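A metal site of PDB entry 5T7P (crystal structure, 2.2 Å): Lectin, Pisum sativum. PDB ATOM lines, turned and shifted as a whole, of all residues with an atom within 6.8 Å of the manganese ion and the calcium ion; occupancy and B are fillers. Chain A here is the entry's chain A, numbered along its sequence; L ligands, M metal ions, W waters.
An oxygen (O2) of the ligand lies within hydrogen-bond range of the backbone NH of Gly 99. An oxygen (O3) of the ligand lies within hydrogen-bond range of the side-chain carboxylate of Asp 81 (2.6 Å). ND2 of Asn 125 sits at hydrogen-bond distance from O3 of the ligand.
The indole nitrogen (NE1) of Trp 128 lies close to the side-chain carboxylate (OD1) of Asp 129 (3.5 Å). The side-chain hydroxyl (OG) of Ser 146 lies close to the side-chain carboxylate (OE1) of Glu 119 (3.4 Å). The side-chain carboxylate (OD2) of Asp 140 sits close to the side-chain carboxylate (OE2) of Glu 119, at 2.6 Å. The backbone carbonyl oxygen of Gly 138 is in hydrogen-bond range of the backbone NH of Glu 119.
Of the 22 residues printed, 4 come within 4 Å of the manganese ion. The nearest printed residue that does not touch the manganese ion is Ser 146 (4.2 Å).
The manganese ion is bound by the side-chain carboxylate of Asp 121 (2.1 Å), the side-chain carboxylate of Asp 129 (2.1 Å), a ring nitrogen (NE2) of His 136 (2.2 Å), the side-chain carboxylate of Glu 119 (2.2 Å), water W1 (2.3 Å) and water W3 (2.3 Å).
O of Phe 123 is bound to the calcium ion (2.3 Å). OD2 of Asp 129 is bound to the calcium ion (2.3 Å). Water W2 is bound to the calcium ion (2.4 Å). OD1 of Asn 125 is bound to the calcium ion. The calcium ion is bound by OD1 of Asp 121, at 2.4 Å. The calcium ion is bound by water W4 (2.4 Å). OD2 of Asp 121 is bound to the calcium ion (2.5 Å).
Water W3 lies within hydrogen-bond range of O of Ile 144 (2.7 Å) and NE1 of Trp 128 (3.5 Å). Water W2 bridges O of Gly 99 (2.7 Å) and NE1 of Trp 128 (2.8 Å).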
ATOM      1  N   ASP A  81     -23.515   0.836  -2.388  1.00  0.00           N
ATOM      2  CA  ASP A  81     -22.294   0.218  -2.779  1.00  0.00           C
ATOM      3  C   ASP A  81     -21.978   0.597  -4.207  1.00  0.00           C
ATOM      4  O   ASP A  81     -20.893   0.449  -4.641  1.00  0.00           O
ATOM      5  CB  ASP A  81     -22.386  -1.281  -2.741  1.00  0.00           C
ATOM      6  CG  ASP A  81     -22.042  -1.838  -1.434  1.00  0.00           C
ATOM      7  OD1 ASP A  81     -20.901  -1.948  -1.173  1.00  0.00           O
ATOM      8  OD2 ASP A  81     -22.935  -2.149  -0.659  1.00  0.00           O
ATOM      9  N   GLY A  98     -24.298  -6.338  -1.592  1.00  0.00           N
ATOM     10  CA  GLY A  98     -23.222  -5.544  -1.015  1.00  0.00           C
ATOM     11  C   GLY A  98     -22.198  -5.173  -2.071  1.00  0.00           C
ATOM     12  O   GLY A  98     -22.545  -4.794  -3.200  1.00  0.00           O
ATOM     13  N   GLY A  99     -20.923  -5.305  -1.730  1.00  0.00           N
ATOM     14  CA  GLY A  99     -19.845  -4.949  -2.640  1.00  0.00           C
ATOM     15  C   GLY A  99     -19.812  -5.766  -3.931  1.00  0.00           C
ATOM     16  O   GLY A  99     -19.071  -5.407  -4.850  1.00  0.00           O
ATOM     17  N   TYR A 100     -20.588  -6.844  -4.007  1.00  0.00           N
ATOM     18  CA  TYR A 100     -20.650  -7.633  -5.236  1.00  0.00           C
ATOM     19  C   TYR A 100     -21.618  -7.073  -6.262  1.00  0.00           C
ATOM     20  O   TYR A 100     -21.686  -7.607  -7.371  1.00  0.00           O
ATOM     21  CB  TYR A 100     -21.006  -9.089  -4.895  1.00  0.00           C
ATOM     22  CG  TYR A 100     -19.888  -9.809  -4.193  1.00  0.00           C
ATOM     23  CD1 TYR A 100     -19.780  -9.775  -2.803  1.00  0.00           C
ATOM     24  CD2 TYR A 100     -18.903 -10.492  -4.932  1.00  0.00           C
ATOM     25  CE1 TYR A 100     -18.728 -10.416  -2.156  1.00  0.00           C
ATOM     26  CE2 TYR A 100     -17.866 -11.127  -4.303  1.00  0.00           C
ATOM     27  CZ  TYR A 100     -17.780 -11.092  -2.912  1.00  0.00           C
ATOM     28  OH  TYR A 100     -16.743 -11.727  -2.284  1.00  0.00           O
ATOM     29  N   LEU A 101     -22.371  -6.035  -5.905  1.00  0.00           N
ATOM     30  CA  LEU A 101     -23.190  -5.264  -6.835  1.00  0.00           C
ATOM     31  C   LEU A 101     -24.254  -6.120  -7.533  1.00  0.00           C
ATOM     32  O   LEU A 101     -24.741  -5.757  -8.611  1.00  0.00           O
ATOM     33  CB  LEU A 101     -22.313  -4.537  -7.884  1.00  0.00           C
ATOM     34  CG  LEU A 101     -21.270  -3.549  -7.333  1.00  0.00           C
ATOM     35  CD1 LEU A 101     -20.264  -3.105  -8.388  1.00  0.00           C
ATOM     36  CD2 LEU A 101     -21.910  -2.315  -6.728  1.00  0.00           C
ATOM     37  N   GLU A 119     -18.955  -0.865 -13.709  1.00  0.00           N
ATOM     38  CA  GLU A 119     -19.332  -0.551 -12.343  1.00  0.00           C
ATOM     39  C   GLU A 119     -18.999   0.899 -12.038  1.00  0.00           C
ATOM     40  O   GLU A 119     -18.013   1.457 -12.543  1.00  0.00           O
ATOM     41  CB  GLU A 119     -18.651  -1.485 -11.323  1.00  0.00           C
ATOM     42  CG  GLU A 119     -17.116  -1.541 -11.352  1.00  0.00           C
ATOM     43  CD  GLU A 119     -16.507  -2.162 -10.098  1.00  0.00           C
ATOM     44  OE1 GLU A 119     -15.681  -1.506  -9.433  1.00  0.00           O
ATOM     45  OE2 GLU A 119     -16.858  -3.304  -9.761  1.00  0.00           O
ATOM     46  N   ASP A 121     -18.516   2.333  -8.627  1.00  0.00           N
ATOM     47  CA  ASP A 121     -18.344   1.649  -7.343  1.00  0.00           C
ATOM     48  C   ASP A 121     -17.995   2.683  -6.275  1.00  0.00           C
ATOM     49  O   ASP A 121     -16.899   3.263  -6.304  1.00  0.00           O
ATOM     50  CB  ASP A 121     -17.241   0.588  -7.482  1.00  0.00           C
ATOM     51  CG  ASP A 121     -17.003  -0.199  -6.215  1.00  0.00           C
ATOM     52  OD1 ASP A 121     -17.483   0.194  -5.133  1.00  0.00           O
ATOM     53  OD2 ASP A 121     -16.304  -1.210  -6.295  1.00  0.00           O
ATOM     54  N   THR A 122     -18.905   2.888  -5.319  1.00  0.00           N
ATOM     55  CA  THR A 122     -18.787   3.970  -4.350  1.00  0.00           C
ATOM     56  C   THR A 122     -18.181   3.541  -3.027  1.00  0.00           C
ATOM     57  O   THR A 122     -17.988   4.395  -2.152  1.00  0.00           O
ATOM     58  CB  THR A 122     -20.141   4.606  -4.090  1.00  0.00           C
ATOM     59  OG1 THR A 122     -21.067   3.612  -3.622  1.00  0.00           O
ATOM     60  CG2 THR A 122     -20.680   5.240  -5.346  1.00  0.00           C
ATOM     61  N   PHE A 123     -17.870   2.266  -2.840  1.00  0.00           N
ATOM     62  CA  PHE A 123     -17.415   1.763  -1.549  1.00  0.00           C
ATOM     63  C   PHE A 123     -16.193   0.865  -1.710  1.00  0.00           C
ATOM     64  O   PHE A 123     -16.221  -0.108  -2.459  1.00  0.00           O
ATOM     65  CB  PHE A 123     -18.518   0.981  -0.831  1.00  0.00           C
ATOM     66  CG  PHE A 123     -18.137   0.556   0.557  1.00  0.00           C
ATOM     67  CD1 PHE A 123     -18.312   1.406   1.649  1.00  0.00           C
ATOM     68  CD2 PHE A 123     -17.581  -0.708   0.787  1.00  0.00           C
ATOM     69  CE1 PHE A 123     -17.951   1.003   2.936  1.00  0.00           C
ATOM     70  CE2 PHE A 123     -17.211  -1.115   2.076  1.00  0.00           C
ATOM     71  CZ  PHE A 123     -17.401  -0.265   3.142  1.00  0.00           C
ATOM     72  N   TYR A 124     -15.151   1.161  -0.945  1.00  0.00           N
ATOM     73  CA  TYR A 124     -13.896   0.431  -1.004  1.00  0.00           C
ATOM     74  C   TYR A 124     -14.046  -0.913  -0.303  1.00  0.00           C
ATOM     75  O   TYR A 124     -14.109  -0.988   0.925  1.00  0.00           O
ATOM     76  CB  TYR A 124     -12.781   1.253  -0.373  1.00  0.00           C
ATOM     77  CG  TYR A 124     -11.493   0.469  -0.181  1.00  0.00           C
ATOM     78  CD1 TYR A 124     -10.722   0.113  -1.274  1.00  0.00           C
ATOM     79  CD2 TYR A 124     -11.056   0.092   1.104  1.00  0.00           C
ATOM     80  CE1 TYR A 124      -9.553  -0.605  -1.121  1.00  0.00           C
ATOM     81  CE2 TYR A 124      -9.858  -0.628   1.271  1.00  0.00           C
ATOM     82  CZ  TYR A 124      -9.113  -0.966   0.135  1.00  0.00           C
ATOM     83  OH  TYR A 124      -7.941  -1.674   0.251  1.00  0.00           O
ATOM     84  N   ASN A 125     -14.094  -1.990  -1.078  1.00  0.00           N
ATOM     85  CA  ASN A 125     -14.010  -3.336  -0.512  1.00  0.00           C
ATOM     86  C   ASN A 125     -12.552  -3.756  -0.542  1.00  0.00           C
ATOM     87  O   ASN A 125     -11.977  -3.949  -1.623  1.00  0.00           O
ATOM     88  CB  ASN A 125     -14.900  -4.306  -1.278  1.00  0.00           C
ATOM     89  CG  ASN A 125     -16.364  -3.926  -1.198  1.00  0.00           C
ATOM     90  OD1 ASN A 125     -16.875  -3.227  -2.067  1.00  0.00           O
ATOM     91  ND2 ASN A 125     -17.028  -4.339  -0.111  1.00  0.00           N
ATOM     92  N   TRP A 128     -10.696  -6.545  -2.852  1.00  0.00           N
ATOM     93  CA  TRP A 128     -10.476  -6.506  -4.301  1.00  0.00           C
ATOM     94  C   TRP A 128     -10.365  -5.117  -4.919  1.00  0.00           C
ATOM     95  O   TRP A 128      -9.846  -5.004  -6.033  1.00  0.00           O
ATOM     96  CB  TRP A 128     -11.587  -7.239  -5.028  1.00  0.00           C
ATOM     97  CG  TRP A 128     -12.966  -6.726  -4.721  1.00  0.00           C
ATOM     98  CD1 TRP A 128     -13.560  -5.616  -5.215  1.00  0.00           C
ATOM     99  CD2 TRP A 128     -13.929  -7.335  -3.843  1.00  0.00           C
ATOM    100  NE1 TRP A 128     -14.833  -5.477  -4.707  1.00  0.00           N
ATOM    101  CE2 TRP A 128     -15.090  -6.526  -3.863  1.00  0.00           C
ATOM    102  CE3 TRP A 128     -13.934  -8.475  -3.040  1.00  0.00           C
ATOM    103  CZ2 TRP A 128     -16.223  -6.820  -3.114  1.00  0.00           C
ATOM    104  CZ3 TRP A 128     -15.071  -8.776  -2.285  1.00  0.00           C
ATOM    105  CH2 TRP A 128     -16.198  -7.961  -2.340  1.00  0.00           C
ATOM    106  N   ASP A 129     -10.893  -4.082  -4.260  1.00  0.00           N
ATOM    107  CA  ASP A 129     -10.982  -2.774  -4.900  1.00  0.00           C
ATOM    108  C   ASP A 129      -9.615  -2.094  -4.984  1.00  0.00           C
ATOM    109  O   ASP A 129      -8.705  -2.448  -4.239  1.00  0.00           O
ATOM    110  CB  ASP A 129     -11.984  -1.898  -4.161  1.00  0.00           C
ATOM    111  CG  ASP A 129     -13.380  -2.046  -4.714  1.00  0.00           C
ATOM    112  OD1 ASP A 129     -13.474  -2.477  -5.876  1.00  0.00           O
ATOM    113  OD2 ASP A 129     -14.380  -1.754  -3.997  1.00  0.00           O
ATOM    114  N   PRO A 130      -9.459  -1.119  -5.876  1.00  0.00           N
ATOM    115  CA  PRO A 130      -8.147  -0.460  -6.032  1.00  0.00           C
ATOM    116  C   PRO A 130      -7.658   0.094  -4.709  1.00  0.00           C
ATOM    117  O   PRO A 130      -8.424   0.637  -3.910  1.00  0.00           O
ATOM    118  CB  PRO A 130      -8.424   0.651  -7.050  1.00  0.00           C
ATOM    119  CG  PRO A 130      -9.576   0.140  -7.855  1.00  0.00           C
ATOM    120  CD  PRO A 130     -10.447  -0.608  -6.856  1.00  0.00           C
ATOM    121  N   HIS A 136     -14.587   4.571  -7.907  1.00  0.00           N
ATOM    122  CA  HIS A 136     -13.962   4.248  -9.186  1.00  0.00           C
ATOM    123  C   HIS A 136     -14.971   3.679 -10.150  1.00  0.00           C
ATOM    124  O   HIS A 136     -15.911   2.973  -9.770  1.00  0.00           O
ATOM    125  CB  HIS A 136     -12.809   3.257  -9.012  1.00  0.00           C
ATOM    126  CG  HIS A 136     -13.204   2.016  -8.282  1.00  0.00           C
ATOM    127  ND1 HIS A 136     -13.258   1.957  -6.906  1.00  0.00           N
ATOM    128  CD2 HIS A 136     -13.572   0.790  -8.724  1.00  0.00           C
ATOM    129  CE1 HIS A 136     -13.621   0.741  -6.541  1.00  0.00           C
ATOM    130  NE2 HIS A 136     -13.818   0.024  -7.623  1.00  0.00           N
ATOM    131  N   ILE A 137     -14.757   3.989 -11.414  1.00  0.00           N
ATOM    132  CA  ILE A 137     -15.398   3.305 -12.513  1.00  0.00           C
ATOM    133  C   ILE A 137     -14.591   2.055 -12.788  1.00  0.00           C
ATOM    134  O   ILE A 137     -13.368   2.054 -12.645  1.00  0.00           O
ATOM    135  CB  ILE A 137     -15.474   4.236 -13.745  1.00  0.00           C
ATOM    136  CG1 ILE A 137     -16.349   5.460 -13.416  1.00  0.00           C
ATOM    137  CG2 ILE A 137     -15.996   3.497 -14.951  1.00  0.00           C
ATOM    138  CD1 ILE A 137     -16.025   6.683 -14.274  1.00  0.00           C
ATOM    139  N   GLY A 138     -15.258   0.961 -13.127  1.00  0.00           N
ATOM    140  CA  GLY A 138     -14.557  -0.276 -13.393  1.00  0.00           C
ATOM    141  C   GLY A 138     -15.188  -1.027 -14.540  1.00  0.00           C
ATOM    142  O   GLY A 138     -16.375  -0.878 -14.822  1.00  0.00           O
ATOM    143  N   ASP A 140     -15.676  -4.952 -15.390  1.00  0.00           N
ATOM    144  CA  ASP A 140     -15.640  -6.206 -14.647  1.00  0.00           C
ATOM    145  C   ASP A 140     -15.932  -7.342 -15.611  1.00  0.00           C
ATOM    146  O   ASP A 140     -16.919  -7.292 -16.358  1.00  0.00           O
ATOM    147  CB  ASP A 140     -16.683  -6.229 -13.542  1.00  0.00           C
ATOM    148  CG  ASP A 140     -16.513  -5.123 -12.529  1.00  0.00           C
ATOM    149  OD1 ASP A 140     -15.460  -4.426 -12.528  1.00  0.00           O
ATOM    150  OD2 ASP A 140     -17.439  -4.993 -11.695  1.00  0.00           O
ATOM    151  N   ILE A 144     -15.732  -9.495  -9.551  1.00  0.00           N
ATOM    152  CA  ILE A 144     -15.931  -8.187  -8.933  1.00  0.00           C
ATOM    153  C   ILE A 144     -14.632  -7.399  -8.867  1.00  0.00           C
ATOM    154  O   ILE A 144     -14.633  -6.212  -8.531  1.00  0.00           O
ATOM    155  CB  ILE A 144     -16.539  -8.330  -7.527  1.00  0.00           C
ATOM    156  CG1 ILE A 144     -17.204  -7.024  -7.055  1.00  0.00           C
ATOM    157  CG2 ILE A 144     -15.465  -8.767  -6.525  1.00  0.00           C
ATOM    158  CD1 ILE A 144     -18.146  -6.368  -8.089  1.00  0.00           C
ATOM    159  N   LYS A 145     -13.509  -8.033  -9.197  1.00  0.00           N
ATOM    160  CA  LYS A 145     -12.218  -7.366  -9.263  1.00  0.00           C
ATOM    161  C   LYS A 145     -12.033  -6.905 -10.706  1.00  0.00           C
ATOM    162  O   LYS A 145     -11.784  -7.729 -11.595  1.00  0.00           O
ATOM    163  CB  LYS A 145     -11.103  -8.314  -8.815  1.00  0.00           C
ATOM    164  CG  LYS A 145      -9.729  -7.675  -8.698  1.00  0.00           C
ATOM    165  CD  LYS A 145      -8.702  -8.736  -8.316  1.00  0.00           C
ATOM    166  CE  LYS A 145      -7.342  -8.138  -7.998  1.00  0.00           C
ATOM    167  NZ  LYS A 145      -6.698  -8.860  -6.844  1.00  0.00           N
ATOM    168  N   SER A 146     -12.182  -5.607 -10.937  1.00  0.00           N
ATOM    169  CA  SER A 146     -12.197  -5.078 -12.280  1.00  0.00           C
ATOM    170  C   SER A 146     -10.870  -5.346 -12.998  1.00  0.00           C
ATOM    171  O   SER A 146      -9.802  -5.248 -12.393  1.00  0.00           O
ATOM    172  CB  SER A 146     -12.459  -3.567 -12.251  1.00  0.00           C
ATOM    173  OG  SER A 146     -13.577  -3.237 -11.412  1.00  0.00           O
ATOM    174  N   THR A 149      -9.694   0.043 -13.945  1.00  0.00           N
ATOM    175  CA  THR A 149     -10.436   0.980 -13.116  1.00  0.00           C
ATOM    176  C   THR A 149      -9.920   2.387 -13.340  1.00  0.00           C
ATOM    177  O   THR A 149      -8.780   2.593 -13.748  1.00  0.00           O
ATOM    178  CB  THR A 149     -10.335   0.655 -11.614  1.00  0.00           C
ATOM    179  OG1 THR A 149      -8.967   0.668 -11.220  1.00  0.00           O
ATOM    180  CG2 THR A 149     -10.961  -0.684 -11.295  1.00  0.00           C
HETATM  181  O1  LIG L   1     -22.079  -5.872   2.792  1.00  0.00           O
HETATM  182  C1  LIG L   1     -20.767  -5.506   3.218  1.00  0.00           C
HETATM  183  C2  LIG L   1     -19.928  -5.127   2.003  1.00  0.00           C
HETATM  184  O2  LIG L   1     -20.048  -6.147   1.003  1.00  0.00           O
HETATM  185  C3  LIG L   1     -20.361  -3.788   1.424  1.00  0.00           C
HETATM  186  O3  LIG L   1     -19.423  -3.357   0.439  1.00  0.00           O
HETATM  187  C4  LIG L   1     -20.473  -2.727   2.522  1.00  0.00           C
HETATM  188  O4  LIG L   1     -21.356  -3.188   3.544  1.00  0.00           O
HETATM  189  C5  LIG L   1     -20.987  -1.415   1.959  1.00  0.00           C
HETATM  190  O5  LIG L   1     -22.419  -1.415   1.980  1.00  0.00           O
HETATM  191  C6  LIG L   1     -20.845  -4.343   4.207  1.00  0.00           C
HETATM  192  O6  LIG L   1     -19.554  -4.059   4.723  1.00  0.00           O
HETATM  193  C7  LIG L   1     -19.416  -3.335   5.871  1.00  0.00           C
HETATM  194  C8  LIG L   1     -19.535  -3.894   7.222  1.00  0.00           C
HETATM  195  C9  LIG L   1     -19.300  -2.684   8.052  1.00  0.00           C
HETATM  196  N1  LIG L   1     -19.082  -1.637   7.227  1.00  0.00           N
HETATM  197  C10 LIG L   1     -19.141  -1.977   5.898  1.00  0.00           C
HETATM  198  C11 LIG L   1     -19.806  -5.193   7.861  1.00  0.00           C
HETATM  199 CL1  LIG L   1     -20.094  -6.682   6.896  1.00  0.00          CL
HETATM  200  C12 LIG L   1     -19.822  -5.221   9.343  1.00  0.00           C
HETATM  201 BR1  LIG L   1     -20.156  -6.843  10.270  1.00  0.00          BR
HETATM  202  C13 LIG L   1     -19.590  -4.045  10.056  1.00  0.00           C
HETATM  203  C14 LIG L   1     -19.341  -2.816   9.441  1.00  0.00           C
HETATM  204 MN    MN M   1     -14.727  -1.935  -7.534  1.00  0.00          MN
HETATM  205 CA    CA M   2     -16.693  -1.757  -3.932  1.00  0.00          CA
HETATM  206  O   HOH W   1     -13.073  -2.782  -8.897  1.00  0.00           O
HETATM  207  O   HOH W   2     -16.975  -3.767  -5.168  1.00  0.00           O
HETATM  208  O   HOH W   3     -15.801  -3.975  -7.714  1.00  0.00           O
HETATM  209  O   HOH W   4     -19.032  -1.454  -3.360  1.00  0.00           O
